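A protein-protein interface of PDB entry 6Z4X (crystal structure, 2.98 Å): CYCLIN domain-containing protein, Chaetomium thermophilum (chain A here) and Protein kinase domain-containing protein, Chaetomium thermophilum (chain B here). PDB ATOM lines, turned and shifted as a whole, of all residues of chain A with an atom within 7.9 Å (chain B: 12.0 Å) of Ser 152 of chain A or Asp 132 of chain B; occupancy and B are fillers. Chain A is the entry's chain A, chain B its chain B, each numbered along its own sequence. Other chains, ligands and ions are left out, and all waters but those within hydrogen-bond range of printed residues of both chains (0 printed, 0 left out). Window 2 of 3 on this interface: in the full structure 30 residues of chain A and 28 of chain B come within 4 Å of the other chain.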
ATOM      1  N   PHE A 141     -17.088   3.365   9.697  1.00  0.00           N
ATOM      2  CA  PHE A 141     -16.666   4.668  10.210  1.00  0.00           C
ATOM      3  C   PHE A 141     -17.702   5.744   9.897  1.00  0.00           C
ATOM      4  O   PHE A 141     -18.112   6.519  10.778  1.00  0.00           O
ATOM      5  CB  PHE A 141     -15.304   5.027   9.615  1.00  0.00           C
ATOM      6  CG  PHE A 141     -14.708   6.288  10.162  1.00  0.00           C
ATOM      7  CD1 PHE A 141     -14.209   6.330  11.453  1.00  0.00           C
ATOM      8  CD2 PHE A 141     -14.624   7.426   9.379  1.00  0.00           C
ATOM      9  CE1 PHE A 141     -13.651   7.489  11.957  1.00  0.00           C
ATOM     10  CE2 PHE A 141     -14.067   8.588   9.877  1.00  0.00           C
ATOM     11  CZ  PHE A 141     -13.580   8.620  11.168  1.00  0.00           C
ATOM     12  N   LYS A 145     -20.187   8.118  12.282  1.00  0.00           N
ATOM     13  CA  LYS A 145     -20.395   9.560  12.155  1.00  0.00           C
ATOM     14  C   LYS A 145     -21.870   9.889  11.938  1.00  0.00           C
ATOM     15  O   LYS A 145     -22.393  10.846  12.522  1.00  0.00           O
ATOM     16  CB  LYS A 145     -19.539  10.127  11.024  1.00  0.00           C
ATOM     17  CG  LYS A 145     -18.069  10.238  11.381  1.00  0.00           C
ATOM     18  CD  LYS A 145     -17.274  10.932  10.291  1.00  0.00           C
ATOM     19  CE  LYS A 145     -15.862  11.236  10.767  1.00  0.00           C
ATOM     20  NZ  LYS A 145     -15.004  11.799   9.687  1.00  0.00           N
ATOM     21  N   ALA A 149     -21.730   9.626  16.486  1.00  0.00           N
ATOM     22  CA  ALA A 149     -20.498   9.224  17.154  1.00  0.00           C
ATOM     23  C   ALA A 149     -19.318   9.559  16.252  1.00  0.00           C
ATOM     24  O   ALA A 149     -19.150   8.955  15.187  1.00  0.00           O
ATOM     25  CB  ALA A 149     -20.522   7.736  17.494  1.00  0.00           C
ATOM     26  N   PHE A 150     -18.502  10.511  16.680  1.00  0.00           N
ATOM     27  CA  PHE A 150     -17.375  10.951  15.873  1.00  0.00           C
ATOM     28  C   PHE A 150     -16.069  10.590  16.565  1.00  0.00           C
ATOM     29  O   PHE A 150     -15.447  11.442  17.213  1.00  0.00           O
ATOM     30  CB  PHE A 150     -17.452  12.454  15.612  1.00  0.00           C
ATOM     31  CG  PHE A 150     -18.682  12.869  14.871  1.00  0.00           C
ATOM     32  CD1 PHE A 150     -18.710  12.837  13.489  1.00  0.00           C
ATOM     33  CD2 PHE A 150     -19.816  13.269  15.554  1.00  0.00           C
ATOM     34  CE1 PHE A 150     -19.843  13.212  12.797  1.00  0.00           C
ATOM     35  CE2 PHE A 150     -20.954  13.646  14.871  1.00  0.00           C
ATOM     36  CZ  PHE A 150     -20.968  13.617  13.487  1.00  0.00           C
ATOM     37  N   PRO A 151     -15.621   9.346  16.440  1.00  0.00           N
ATOM     38  CA  PRO A 151     -14.387   8.924  17.104  1.00  0.00           C
ATOM     39  C   PRO A 151     -13.157   9.401  16.342  1.00  0.00           C
ATOM     40  O   PRO A 151     -13.235   9.898  15.219  1.00  0.00           O
ATOM     41  CB  PRO A 151     -14.496   7.400  17.077  1.00  0.00           C
ATOM     42  CG  PRO A 151     -15.239   7.130  15.797  1.00  0.00           C
ATOM     43  CD  PRO A 151     -16.213   8.269  15.626  1.00  0.00           C
ATOM     44  N   SER A 152     -12.004   9.238  16.983  1.00  0.00           N
ATOM     45  CA  SER A 152     -10.736   9.526  16.331  1.00  0.00           C
ATOM     46  C   SER A 152     -10.399   8.400  15.361  1.00  0.00           C
ATOM     47  O   SER A 152     -10.515   7.218  15.704  1.00  0.00           O
ATOM     48  CB  SER A 152      -9.624   9.692  17.366  1.00  0.00           C
ATOM     49  OG  SER A 152      -9.207   8.434  17.865  1.00  0.00           O
ATOM     50  N   ILE A 153      -9.996   8.767  14.143  1.00  0.00           N
ATOM     51  CA  ILE A 153      -9.693   7.758  13.134  1.00  0.00           C
ATOM     52  C   ILE A 153      -8.590   6.828  13.617  1.00  0.00           C
ATOM     53  O   ILE A 153      -8.581   5.635  13.284  1.00  0.00           O
ATOM     54  CB  ILE A 153      -9.323   8.437  11.799  1.00  0.00           C
ATOM     55  CG1 ILE A 153      -9.193   7.392  10.690  1.00  0.00           C
ATOM     56  CG2 ILE A 153      -8.042   9.251  11.944  1.00  0.00           C
ATOM     57  CD1 ILE A 153     -10.473   6.626  10.428  1.00  0.00           C
ATOM     58  N   SER A 154      -7.653   7.347  14.415  1.00  0.00           N
ATOM     59  CA  SER A 154      -6.571   6.511  14.928  1.00  0.00           C
ATOM     60  C   SER A 154      -7.104   5.437  15.868  1.00  0.00           C
ATOM     61  O   SER A 154      -6.721   4.266  15.766  1.00  0.00           O
ATOM     62  CB  SER A 154      -5.522   7.377  15.629  1.00  0.00           C
ATOM     63  OG  SER A 154      -6.066   8.013  16.771  1.00  0.00           O
ATOM     64  N   ASP A 155      -7.991   5.814  16.795  1.00  0.00           N
ATOM     65  CA  ASP A 155      -8.578   4.824  17.692  1.00  0.00           C
ATOM     66  C   ASP A 155      -9.381   3.791  16.916  1.00  0.00           C
ATOM     67  O   ASP A 155      -9.377   2.602  17.259  1.00  0.00           O
ATOM     68  CB  ASP A 155      -9.461   5.510  18.736  1.00  0.00           C
ATOM     69  CG  ASP A 155      -8.661   6.299  19.749  1.00  0.00           C
ATOM     70  OD1 ASP A 155      -7.502   5.920  20.015  1.00  0.00           O
ATOM     71  OD2 ASP A 155      -9.194   7.298  20.279  1.00  0.00           O
ATOM     72  N   PHE A 156     -10.079   4.227  15.866  1.00  0.00           N
ATOM     73  CA  PHE A 156     -10.845   3.299  15.040  1.00  0.00           C
ATOM     74  C   PHE A 156      -9.928   2.276  14.379  1.00  0.00           C
ATOM     75  O   PHE A 156     -10.140   1.059  14.493  1.00  0.00           O
ATOM     76  CB  PHE A 156     -11.637   4.088  13.995  1.00  0.00           C
ATOM     77  CG  PHE A 156     -12.623   3.264  13.224  1.00  0.00           C
ATOM     78  CD1 PHE A 156     -13.915   3.093  13.688  1.00  0.00           C
ATOM     79  CD2 PHE A 156     -12.262   2.674  12.026  1.00  0.00           C
ATOM     80  CE1 PHE A 156     -14.827   2.338  12.975  1.00  0.00           C
ATOM     81  CE2 PHE A 156     -13.169   1.919  11.309  1.00  0.00           C
ATOM     82  CZ  PHE A 156     -14.453   1.751  11.785  1.00  0.00           C
ATOM     83  N   ALA A 157      -8.881   2.755  13.701  1.00  0.00           N
ATOM     84  CA  ALA A 157      -7.941   1.844  13.059  1.00  0.00           C
ATOM     85  C   ALA A 157      -7.287   0.923  14.079  1.00  0.00           C
ATOM     86  O   ALA A 157      -7.031  -0.252  13.789  1.00  0.00           O
ATOM     87  CB  ALA A 157      -6.883   2.639  12.294  1.00  0.00           C
ATOM     88  N   LYS A 158      -7.015   1.434  15.283  1.00  0.00           N
ATOM     89  CA  LYS A 158      -6.452   0.590  16.329  1.00  0.00           C
ATOM     90  C   LYS A 158      -7.411  -0.536  16.685  1.00  0.00           C
ATOM     91  O   LYS A 158      -7.031  -1.712  16.702  1.00  0.00           O
ATOM     92  CB  LYS A 158      -6.126   1.429  17.567  1.00  0.00           C
ATOM     93  CG  LYS A 158      -5.598   0.615  18.746  1.00  0.00           C
ATOM     94  CD  LYS A 158      -5.339   1.486  19.972  1.00  0.00           C
ATOM     95  CE  LYS A 158      -6.623   2.123  20.489  1.00  0.00           C
ATOM     96  NZ  LYS A 158      -6.396   2.891  21.749  1.00  0.00           N
ATOM     97  N   THR A 159      -8.669  -0.191  16.967  1.00  0.00           N
ATOM     98  CA  THR A 159      -9.643  -1.209  17.343  1.00  0.00           C
ATOM     99  C   THR A 159      -9.852  -2.223  16.227  1.00  0.00           C
ATOM    100  O   THR A 159     -10.237  -3.365  16.497  1.00  0.00           O
ATOM    101  CB  THR A 159     -10.974  -0.560  17.728  1.00  0.00           C
ATOM    102  OG1 THR A 159     -11.493   0.175  16.613  1.00  0.00           O
ATOM    103  CG2 THR A 159     -10.789   0.382  18.913  1.00  0.00           C
ATOM    104  N   PRO A 165      -4.195   4.655   9.282  1.00  0.00           N
ATOM    105  CA  PRO A 165      -5.576   5.156   9.347  1.00  0.00           C
ATOM    106  C   PRO A 165      -6.026   5.847   8.073  1.00  0.00           C
ATOM    107  O   PRO A 165      -7.224   5.824   7.764  1.00  0.00           O
ATOM    108  CB  PRO A 165      -5.543   6.124  10.538  1.00  0.00           C
ATOM    109  CG  PRO A 165      -4.113   6.548  10.638  1.00  0.00           C
ATOM    110  CD  PRO A 165      -3.301   5.357  10.219  1.00  0.00           C
ATOM    111  N   LEU A 169      -9.711   6.926   5.657  1.00  0.00           N
ATOM    112  CA  LEU A 169     -10.157   8.257   5.254  1.00  0.00           C
ATOM    113  C   LEU A 169     -10.233   8.372   3.736  1.00  0.00           C
ATOM    114  O   LEU A 169     -11.132   9.029   3.197  1.00  0.00           O
ATOM    115  CB  LEU A 169      -9.217   9.321   5.821  1.00  0.00           C
ATOM    116  CG  LEU A 169      -9.039   9.378   7.338  1.00  0.00           C
ATOM    117  CD1 LEU A 169      -8.042  10.465   7.715  1.00  0.00           C
ATOM    118  CD2 LEU A 169     -10.371   9.612   8.026  1.00  0.00           C
ATOM    119  N   GLU A 172     -13.722   7.768   2.701  1.00  0.00           N
ATOM    120  CA  GLU A 172     -14.848   8.416   3.363  1.00  0.00           C
ATOM    121  C   GLU A 172     -15.667   9.235   2.374  1.00  0.00           C
ATOM    122  O   GLU A 172     -16.797   8.859   2.043  1.00  0.00           O
ATOM    123  CB  GLU A 172     -14.373   9.301   4.519  1.00  0.00           C
ATOM    124  CG  GLU A 172     -15.522   9.827   5.374  1.00  0.00           C
ATOM    125  CD  GLU A 172     -15.059  10.691   6.530  1.00  0.00           C
ATOM    126  OE1 GLU A 172     -15.648  10.578   7.626  1.00  0.00           O
ATOM    127  OE2 GLU A 172     -14.099  11.471   6.349  1.00  0.00           O
ATOM    128  N   VAL B 126     -12.294  22.197   3.495  1.00  0.00           N
ATOM    129  CA  VAL B 126     -11.669  21.279   4.436  1.00  0.00           C
ATOM    130  C   VAL B 126     -11.034  22.056   5.576  1.00  0.00           C
ATOM    131  O   VAL B 126     -10.471  23.142   5.381  1.00  0.00           O
ATOM    132  CB  VAL B 126     -10.629  20.399   3.722  1.00  0.00           C
ATOM    133  CG1 VAL B 126      -9.738  19.701   4.737  1.00  0.00           C
ATOM    134  CG2 VAL B 126     -11.323  19.379   2.834  1.00  0.00           C
ATOM    135  N   GLN B 127     -11.125  21.503   6.781  1.00  0.00           N
ATOM    136  CA  GLN B 127     -10.533  22.108   7.968  1.00  0.00           C
ATOM    137  C   GLN B 127      -9.255  21.339   8.283  1.00  0.00           C
ATOM    138  O   GLN B 127      -9.307  20.204   8.769  1.00  0.00           O
ATOM    139  CB  GLN B 127     -11.506  22.093   9.144  1.00  0.00           C
ATOM    140  CG  GLN B 127     -11.075  22.992  10.294  1.00  0.00           C
ATOM    141  CD  GLN B 127     -10.983  24.450   9.880  1.00  0.00           C
ATOM    142  OE1 GLN B 127     -11.744  24.916   9.030  1.00  0.00           O
ATOM    143  NE2 GLN B 127     -10.045  25.177  10.479  1.00  0.00           N
ATOM    144  N   ALA B 128      -8.108  21.958   7.997  1.00  0.00           N
ATOM    145  CA  ALA B 128      -6.823  21.310   8.230  1.00  0.00           C
ATOM    146  C   ALA B 128      -6.620  20.927   9.690  1.00  0.00           C
ATOM    147  O   ALA B 128      -5.817  20.032   9.979  1.00  0.00           O
ATOM    148  CB  ALA B 128      -5.686  22.220   7.768  1.00  0.00           C
ATOM    149  N   GLN B 129      -7.314  21.590  10.617  1.00  0.00           N
ATOM    150  CA  GLN B 129      -7.143  21.291  12.034  1.00  0.00           C
ATOM    151  C   GLN B 129      -7.720  19.932  12.419  1.00  0.00           C
ATOM    152  O   GLN B 129      -7.294  19.359  13.429  1.00  0.00           O
ATOM    153  CB  GLN B 129      -7.781  22.398  12.876  1.00  0.00           C
ATOM    154  CG  GLN B 129      -7.168  22.572  14.259  1.00  0.00           C
ATOM    155  CD  GLN B 129      -7.653  21.545  15.262  1.00  0.00           C
ATOM    156  OE1 GLN B 129      -8.856  21.337  15.424  1.00  0.00           O
ATOM    157  NE2 GLN B 129      -6.715  20.900  15.949  1.00  0.00           N
ATOM    158  N   TYR B 130      -8.662  19.397  11.643  1.00  0.00           N
ATOM    159  CA  TYR B 130      -9.347  18.153  11.979  1.00  0.00           C
ATOM    160  C   TYR B 130      -8.750  17.006  11.172  1.00  0.00           C
ATOM    161  O   TYR B 130      -8.824  17.005   9.937  1.00  0.00           O
ATOM    162  CB  TYR B 130     -10.846  18.267  11.712  1.00  0.00           C
ATOM    163  CG  TYR B 130     -11.676  17.286  12.505  1.00  0.00           C
ATOM    164  CD1 TYR B 130     -11.544  17.195  13.885  1.00  0.00           C
ATOM    165  CD2 TYR B 130     -12.586  16.448  11.876  1.00  0.00           C
ATOM    166  CE1 TYR B 130     -12.299  16.301  14.616  1.00  0.00           C
ATOM    167  CE2 TYR B 130     -13.345  15.549  12.598  1.00  0.00           C
ATOM    168  CZ  TYR B 130     -13.198  15.479  13.968  1.00  0.00           C
ATOM    169  OH  TYR B 130     -13.951  14.588  14.699  1.00  0.00           O
ATOM    170  N   LYS B 131      -8.170  16.032  11.870  1.00  0.00           N
ATOM    171  CA  LYS B 131      -7.513  14.895  11.245  1.00  0.00           C
ATOM    172  C   LYS B 131      -8.383  13.645  11.185  1.00  0.00           C
ATOM    173  O   LYS B 131      -7.901  12.596  10.751  1.00  0.00           O
ATOM    174  CB  LYS B 131      -6.209  14.574  11.984  1.00  0.00           C
ATOM    175  CG  LYS B 131      -5.306  15.781  12.185  1.00  0.00           C
ATOM    176  CD  LYS B 131      -3.879  15.373  12.507  1.00  0.00           C
ATOM    177  CE  LYS B 131      -2.986  16.597  12.641  1.00  0.00           C
ATOM    178  NZ  LYS B 131      -2.906  17.371  11.370  1.00  0.00           N
ATOM    179  N   ASP B 132      -9.646  13.725  11.609  1.00  0.00           N
ATOM    180  CA  ASP B 132     -10.527  12.564  11.645  1.00  0.00           C
ATOM    181  C   ASP B 132     -11.506  12.531  10.476  1.00  0.00           C
ATOM    182  O   ASP B 132     -12.622  12.022  10.618  1.00  0.00           O
ATOM    183  CB  ASP B 132     -11.291  12.523  12.967  1.00  0.00           C
ATOM    184  CG  ASP B 132     -10.385  12.287  14.154  1.00  0.00           C
ATOM    185  OD1 ASP B 132      -9.205  11.934  13.938  1.00  0.00           O
ATOM    186  OD2 ASP B 132     -10.853  12.448  15.302  1.00  0.00           O
ATOM    187  N   GLY B 133     -11.107  13.049   9.318  1.00  0.00           N
ATOM    188  CA  GLY B 133     -11.961  12.981   8.150  1.00  0.00           C
ATOM    189  C   GLY B 133     -12.971  14.107   8.084  1.00  0.00           C
ATOM    190  O   GLY B 133     -12.662  15.252   8.430  1.00  0.00           O
ATOM    191  N   MET B 134     -14.182  13.792   7.630  1.00  0.00           N
ATOM    192  CA  MET B 134     -15.216  14.806   7.467  1.00  0.00           C
ATOM    193  C   MET B 134     -15.633  15.387   8.815  1.00  0.00           C
ATOM    194  O   MET B 134     -15.841  14.659   9.789  1.00  0.00           O
ATOM    195  CB  MET B 134     -16.424  14.211   6.746  1.00  0.00           C
ATOM    196  CG  MET B 134     -17.425  15.240   6.259  1.00  0.00           C
ATOM    197  SD  MET B 134     -18.606  14.503   5.117  1.00  0.00           S
ATOM    198  CE  MET B 134     -17.489  13.662   3.993  1.00  0.00           C
ATOM    199  N   ALA B 135     -15.767  16.710   8.857  1.00  0.00           N
ATOM    200  CA  ALA B 135     -16.060  17.398  10.102  1.00  0.00           C
ATOM    201  C   ALA B 135     -17.463  17.056  10.606  1.00  0.00           C
ATOM    202  O   ALA B 135     -18.387  16.856   9.814  1.00  0.00           O
ATOM    203  CB  ALA B 135     -15.929  18.908   9.920  1.00  0.00           C
ATOM    204  N   PRO B 136     -17.644  16.992  11.929  1.00  0.00           N
ATOM    205  CA  PRO B 136     -18.968  16.641  12.466  1.00  0.00           C
ATOM    206  C   PRO B 136     -20.063  17.605  12.056  1.00  0.00           C
ATOM    207  O   PRO B 136     -21.202  17.177  11.830  1.00  0.00           O
ATOM    208  CB  PRO B 136     -18.739  16.657  13.985  1.00  0.00           C
ATOM    209  CG  PRO B 136     -17.278  16.396  14.143  1.00  0.00           C
ATOM    210  CD  PRO B 136     -16.626  17.092  12.987  1.00  0.00           C
ATOM    211  N   ASP B 137     -19.761  18.900  11.966  1.00  0.00           N
ATOM    212  CA  ASP B 137     -20.790  19.854  11.563  1.00  0.00           C
ATOM    213  C   ASP B 137     -21.241  19.594  10.130  1.00  0.00           C
ATOM    214  O   ASP B 137     -22.435  19.698   9.822  1.00  0.00           O
ATOM    215  CB  ASP B 137     -20.275  21.286  11.729  1.00  0.00           C
ATOM    216  CG  ASP B 137     -19.018  21.556  10.922  1.00  0.00           C
ATOM    217  OD1 ASP B 137     -18.514  20.623  10.261  1.00  0.00           O
ATOM    218  OD2 ASP B 137     -18.528  22.705  10.958  1.00  0.00           O
ATOM    219  N   ALA B 138     -20.308  19.213   9.253  1.00  0.00           N
ATOM    220  CA  ALA B 138     -20.670  18.898   7.876  1.00  0.00           C
ATOM    221  C   ALA B 138     -21.632  17.718   7.817  1.00  0.00           C
ATOM    222  O   ALA B 138     -22.683  17.788   7.166  1.00  0.00           O
ATOM    223  CB  ALA B 138     -19.409  18.607   7.060  1.00  0.00           C
ATOM    224  N   VAL B 139     -21.292  16.621   8.500  1.00  0.00           N
ATOM    225  CA  VAL B 139     -22.162  15.448   8.514  1.00  0.00           C
ATOM    226  C   VAL B 139     -23.517  15.797   9.116  1.00  0.00           C
ATOM    227  O   VAL B 139     -24.569  15.401   8.595  1.00  0.00           O
ATOM    228  CB  VAL B 139     -21.487  14.291   9.276  1.00  0.00           C
ATOM    229  CG1 VAL B 139     -22.455  13.133   9.447  1.00  0.00           C
ATOM    230  CG2 VAL B 139     -20.228  13.842   8.552  1.00  0.00           C
ATOM    231  N   ARG B 140     -23.512  16.530  10.231  1.00  0.00           N
ATOM    232  CA  ARG B 140     -24.757  16.851  10.919  1.00  0.00           C
ATOM    233  C   ARG B 140     -25.678  17.675  10.032  1.00  0.00           C
ATOM    234  O   ARG B 140     -26.882  17.402   9.946  1.00  0.00           O
ATOM    235  CB  ARG B 140     -24.453  17.580  12.228  1.00  0.00           C
ATOM    236  CG  ARG B 140     -23.965  16.649  13.316  1.00  0.00           C
ATOM    237  CD  ARG B 140     -23.331  17.379  14.482  1.00  0.00           C
ATOM    238  NE  ARG B 140     -23.006  16.440  15.553  1.00  0.00           N
ATOM    239  CZ  ARG B 140     -22.067  16.642  16.472  1.00  0.00           C
ATOM    240  NH1 ARG B 140     -21.340  17.753  16.453  1.00  0.00           N
ATOM    241  NH2 ARG B 140     -21.847  15.722  17.403  1.00  0.00           N
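Among the printed residues, merely in contact across the chains: Phe 141 of chain A with Asp 132 of chain B (3.6 Å), Lys 145 of chain A with Gly 133 of chain B (3.5 Å), Lys 145 of chain A with Val 139 of chain B (3.8 Å), Phe 150 of chain A with Pro 136 of chain B (3.6 Å), Phe 150 of chain A with Arg 140 of chain B (3.4 Å), Ser 152 of chain A with Asp 132 of chain B (3.1 Å), Ile 153 of chain A with Lys 131 of chain B (3.6 Å), Leu 169 of chain A with Lys 131 of chain B (3.7 Å), Leu 169 of chain A with Asp 132 of chain B (3.98 Å), Leu 169 of chain A with Gly 133 of chain B (3.7 Å) and Glu 172 of chain A with Gly 133 of chain B (3.2 Å).
The side-chain amino group of Lys 145 of chain A is in hydrogen-bond range of the backbone carbonyl oxygen of Met 134 of chain B (3.0 Å).
The side-chain amino group (NZ) of Lys 145 of chain A lies within hydrogen-bond range of the backbone carbonyl oxygen (O) of Asp 132 of chain B (2.6 Å).
The backbone NH (N) of Met 134 of chain B sits at hydrogen-bond distance from the side-chain carboxylate (OE2) of Glu 172 of chain A, at 2.7 Å.
N of Ile 153 of chain A lies within hydrogen-bond range of OD1 of Asp 132 of chain B, at 3.3 Å.
O of Pro 151 of chain A sits close to OD2 of Asp 132 of chain B.
The side-chain hydroxyl (OG) of Ser 152 of chain A lies within hydrogen-bond range of the side-chain carboxylate (OD2) of Asp 155 of chain A, at 2.7 Å.
NZ of Lys 145 of chain A lies within salt-bridge range of OE1 of Glu 172 of chain A.
OG of Ser 152 of chain A sits at hydrogen-bond distance from OG of Ser 154 of chain A, 3.4 Å away.
Hydrophobic or aromatic side chains of chain B that line the printed part of chain A: Met 134, Pro 136 and Val 139.
Of the 16 printed residues of chain A, 8 touch a printed residue of chain B.
Printed residues of chain A that touch a printed residue of chain B: Phe 141, Lys 145, Phe 150, Pro 151, Ser 152, Ile 153, Leu 169 and Glu 172.
Hydrophobic or aromatic side chains of chain A within 4 Å of the printed part of chain B: Phe 141, Phe 150, Ile 153 and Leu 169.
Among the printed residues, 16 pairs touch across the chains.
Among the printed residues, no Asp or Glu carboxylate lies within 4 Å of a Lys or Arg side-chain nitrogen of the other chain.
Ser 152 of chain A touches one residue of chain B.
Asp 132 of chain B touches just these residues of chain A: Phe 141, Lys 145, Pro 151, Ser 152, Ile 153 and Leu 169.
Ile 153 of chain A touches just these residues of chain B: Lys 131 (3.6 Å) and Asp 132 (3.3 Å).
No residue of chain B comes within 4 Å of Ser 154 of chain A.
No residue of chain B comes within 4 Å of Phe 156 of chain A.
Printed residues of chain A within 4 Å of Met 134 of chain B: Lys 145 and Glu 172.
Of the printed residues of chain A, Val 139 of chain B touches Lys 145 (3.8 Å).
Of the printed residues of chain B, Phe 141 of chain A touches Asp 132.
Gln 127 of chain B touches none of the printed residues of chain A.
The nearest residue of chain B that does not touch Ser 152 of chain A is Tyr 130 of chain B (6.1 Å).
The nearest residue of chain A that does not touch Asp 132 of chain B is Glu 172 of chain A (4.5 Å).
The nearest printed residue of chain B that does not touch Lys 145 of chain A is Tyr 130 of chain B (5.0 Å).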
